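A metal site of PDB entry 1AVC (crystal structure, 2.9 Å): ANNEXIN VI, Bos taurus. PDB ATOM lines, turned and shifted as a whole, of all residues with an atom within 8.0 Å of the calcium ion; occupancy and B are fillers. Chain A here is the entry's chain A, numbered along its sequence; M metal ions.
Residues that only touch the calcium ion: Glu 449 (3.4 Å).
The nearest printed residue that does not touch the calcium ion is Ala 451 (4.2 Å).
The calcium ion is bound by the backbone carbonyl oxygen (O) of Gly 452 (2.5 Å), the backbone carbonyl oxygen (O) of Gly 450 (2.5 Å), the backbone carbonyl oxygen (O) of Met 448 (2.6 Å) and the side-chain carboxylate (OD1) of Asp 492 (2.7 Å).
Slightly farther from the calcium ion lies the side-chain carboxylate (OD2) of Asp 492 (3.0 Å).
The side-chain carboxylate (OD2) of Asp 492 lies within hydrogen-bond range of the side-chain hydroxyl (OG1) of Thr 453, 2.5 Å away.
The side-chain carboxylate of Glu 449 lies within salt-bridge range of the side-chain amino group of Lys 446 (3.1 Å).
The side-chain carboxylate (OE1) of Glu 449 lies within salt-bridge range of the side-chain amino group (NZ) of Lys 445 (3.0 Å).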
ATOM      1  N   LEU A 444      10.013 -24.655 -31.088  1.00  0.00           N
ATOM      2  CA  LEU A 444      10.226 -24.700 -29.643  1.00  0.00           C
ATOM      3  C   LEU A 444       8.904 -24.853 -28.892  1.00  0.00           C
ATOM      4  O   LEU A 444       8.818 -25.620 -27.935  1.00  0.00           O
ATOM      5  CB  LEU A 444      10.941 -23.441 -29.174  1.00  0.00           C
ATOM      6  CG  LEU A 444      12.390 -23.275 -29.640  1.00  0.00           C
ATOM      7  CD1 LEU A 444      12.766 -21.805 -29.641  1.00  0.00           C
ATOM      8  CD2 LEU A 444      13.306 -24.063 -28.725  1.00  0.00           C
ATOM      9  N   LYS A 445       7.888 -24.121 -29.329  1.00  0.00           N
ATOM     10  CA  LYS A 445       6.581 -24.168 -28.695  1.00  0.00           C
ATOM     11  C   LYS A 445       5.952 -25.551 -28.783  1.00  0.00           C
ATOM     12  O   LYS A 445       5.358 -26.043 -27.827  1.00  0.00           O
ATOM     13  CB  LYS A 445       5.650 -23.133 -29.335  1.00  0.00           C
ATOM     14  CG  LYS A 445       4.252 -23.097 -28.738  1.00  0.00           C
ATOM     15  CD  LYS A 445       3.213 -23.588 -29.743  1.00  0.00           C
ATOM     16  CE  LYS A 445       1.808 -23.334 -29.253  1.00  0.00           C
ATOM     17  NZ  LYS A 445       1.490 -24.128 -28.030  1.00  0.00           N
ATOM     18  N   LYS A 446       6.076 -26.181 -29.947  1.00  0.00           N
ATOM     19  CA  LYS A 446       5.521 -27.510 -30.169  1.00  0.00           C
ATOM     20  C   LYS A 446       6.226 -28.553 -29.305  1.00  0.00           C
ATOM     21  O   LYS A 446       5.588 -29.432 -28.728  1.00  0.00           O
ATOM     22  CB  LYS A 446       5.642 -27.906 -31.643  1.00  0.00           C
ATOM     23  CG  LYS A 446       4.902 -26.984 -32.591  1.00  0.00           C
ATOM     24  CD  LYS A 446       4.008 -27.778 -33.541  1.00  0.00           C
ATOM     25  CE  LYS A 446       2.698 -27.053 -33.802  1.00  0.00           C
ATOM     26  NZ  LYS A 446       2.176 -26.390 -32.578  1.00  0.00           N
ATOM     27  N   ALA A 447       7.543 -28.431 -29.210  1.00  0.00           N
ATOM     28  CA  ALA A 447       8.357 -29.360 -28.426  1.00  0.00           C
ATOM     29  C   ALA A 447       7.972 -29.346 -26.955  1.00  0.00           C
ATOM     30  O   ALA A 447       8.160 -30.337 -26.249  1.00  0.00           O
ATOM     31  CB  ALA A 447       9.831 -29.018 -28.588  1.00  0.00           C
ATOM     32  N   MET A 448       7.442 -28.218 -26.490  1.00  0.00           N
ATOM     33  CA  MET A 448       7.045 -28.076 -25.093  1.00  0.00           C
ATOM     34  C   MET A 448       5.539 -28.205 -24.864  1.00  0.00           C
ATOM     35  O   MET A 448       5.076 -28.135 -23.716  1.00  0.00           O
ATOM     36  CB  MET A 448       7.519 -26.727 -24.549  1.00  0.00           C
ATOM     37  CG  MET A 448       9.024 -26.562 -24.521  1.00  0.00           C
ATOM     38  SD  MET A 448       9.536 -24.982 -23.841  1.00  0.00           S
ATOM     39  CE  MET A 448       9.336 -23.916 -25.262  1.00  0.00           C
ATOM     40  N   GLU A 449       4.779 -28.385 -25.934  1.00  0.00           N
ATOM     41  CA  GLU A 449       3.326 -28.518 -25.813  1.00  0.00           C
ATOM     42  C   GLU A 449       2.910 -29.984 -25.709  1.00  0.00           C
ATOM     43  O   GLU A 449       3.528 -30.858 -26.332  1.00  0.00           O
ATOM     44  CB  GLU A 449       2.634 -27.873 -27.013  1.00  0.00           C
ATOM     45  CG  GLU A 449       2.598 -28.730 -28.274  1.00  0.00           C
ATOM     46  CD  GLU A 449       2.031 -27.999 -29.460  1.00  0.00           C
ATOM     47  OE1 GLU A 449       1.848 -26.770 -29.357  1.00  0.00           O
ATOM     48  OE2 GLU A 449       1.772 -28.644 -30.492  1.00  0.00           O
ATOM     49  N   GLY A 450       1.881 -30.236 -24.918  1.00  0.00           N
ATOM     50  CA  GLY A 450       1.376 -31.587 -24.713  1.00  0.00           C
ATOM     51  C   GLY A 450       2.101 -32.315 -23.605  1.00  0.00           C
ATOM     52  O   GLY A 450       2.762 -31.687 -22.782  1.00  0.00           O
ATOM     53  N   ALA A 451       2.006 -33.643 -23.576  1.00  0.00           N
ATOM     54  CA  ALA A 451       2.679 -34.421 -22.529  1.00  0.00           C
ATOM     55  C   ALA A 451       4.113 -34.744 -22.931  1.00  0.00           C
ATOM     56  O   ALA A 451       4.356 -35.176 -24.056  1.00  0.00           O
ATOM     57  CB  ALA A 451       1.903 -35.712 -22.259  1.00  0.00           C
ATOM     58  N   GLY A 452       5.053 -34.512 -22.019  1.00  0.00           N
ATOM     59  CA  GLY A 452       6.446 -34.791 -22.310  1.00  0.00           C
ATOM     60  C   GLY A 452       7.144 -33.668 -23.055  1.00  0.00           C
ATOM     61  O   GLY A 452       6.508 -32.727 -23.492  1.00  0.00           O
ATOM     62  N   THR A 453       8.456 -33.771 -23.211  1.00  0.00           N
ATOM     63  CA  THR A 453       9.219 -32.739 -23.906  1.00  0.00           C
ATOM     64  C   THR A 453      10.015 -33.339 -25.059  1.00  0.00           C
ATOM     65  O   THR A 453      10.575 -34.424 -24.935  1.00  0.00           O
ATOM     66  CB  THR A 453      10.200 -32.028 -22.963  1.00  0.00           C
ATOM     67  OG1 THR A 453       9.472 -31.392 -21.903  1.00  0.00           O
ATOM     68  CG2 THR A 453      11.007 -30.978 -23.716  1.00  0.00           C
ATOM     69  N   ASP A 454      10.056 -32.635 -26.182  1.00  0.00           N
ATOM     70  CA  ASP A 454      10.806 -33.103 -27.346  1.00  0.00           C
ATOM     71  C   ASP A 454      12.251 -32.653 -27.148  1.00  0.00           C
ATOM     72  O   ASP A 454      12.783 -31.886 -27.955  1.00  0.00           O
ATOM     73  CB  ASP A 454      10.243 -32.514 -28.633  1.00  0.00           C
ATOM     74  CG  ASP A 454      10.934 -33.053 -29.871  1.00  0.00           C
ATOM     75  OD1 ASP A 454      12.005 -33.683 -29.738  1.00  0.00           O
ATOM     76  OD2 ASP A 454      10.416 -32.841 -30.989  1.00  0.00           O
ATOM     77  N   SER A 491       8.336 -24.019 -17.646  1.00  0.00           N
ATOM     78  CA  SER A 491       7.025 -24.656 -17.508  1.00  0.00           C
ATOM     79  C   SER A 491       6.995 -26.097 -17.985  1.00  0.00           C
ATOM     80  O   SER A 491       6.195 -26.892 -17.484  1.00  0.00           O
ATOM     81  CB  SER A 491       5.972 -23.840 -18.262  1.00  0.00           C
ATOM     82  OG  SER A 491       5.685 -22.636 -17.588  1.00  0.00           O
ATOM     83  N   ASP A 492       7.849 -26.454 -18.941  1.00  0.00           N
ATOM     84  CA  ASP A 492       7.863 -27.807 -19.470  1.00  0.00           C
ATOM     85  C   ASP A 492       9.073 -28.646 -19.072  1.00  0.00           C
ATOM     86  O   ASP A 492       9.060 -29.870 -19.218  1.00  0.00           O
ATOM     87  CB  ASP A 492       7.740 -27.787 -20.986  1.00  0.00           C
ATOM     88  CG  ASP A 492       7.155 -29.072 -21.543  1.00  0.00           C
ATOM     89  OD1 ASP A 492       6.067 -29.469 -21.081  1.00  0.00           O
ATOM     90  OD2 ASP A 492       7.778 -29.671 -22.441  1.00  0.00           O
ATOM     91  N   THR A 493      10.125 -27.997 -18.592  1.00  0.00           N
ATOM     92  CA  THR A 493      11.327 -28.715 -18.191  1.00  0.00           C
ATOM     93  C   THR A 493      11.765 -28.367 -16.780  1.00  0.00           C
ATOM     94  O   THR A 493      11.181 -27.495 -16.133  1.00  0.00           O
ATOM     95  CB  THR A 493      12.498 -28.432 -19.154  1.00  0.00           C
ATOM     96  OG1 THR A 493      12.720 -27.019 -19.234  1.00  0.00           O
ATOM     97  CG2 THR A 493      12.185 -28.973 -20.543  1.00  0.00           C
HETATM   98 CA    CA M   1       5.054 -30.676 -23.220  1.00  0.00          CA
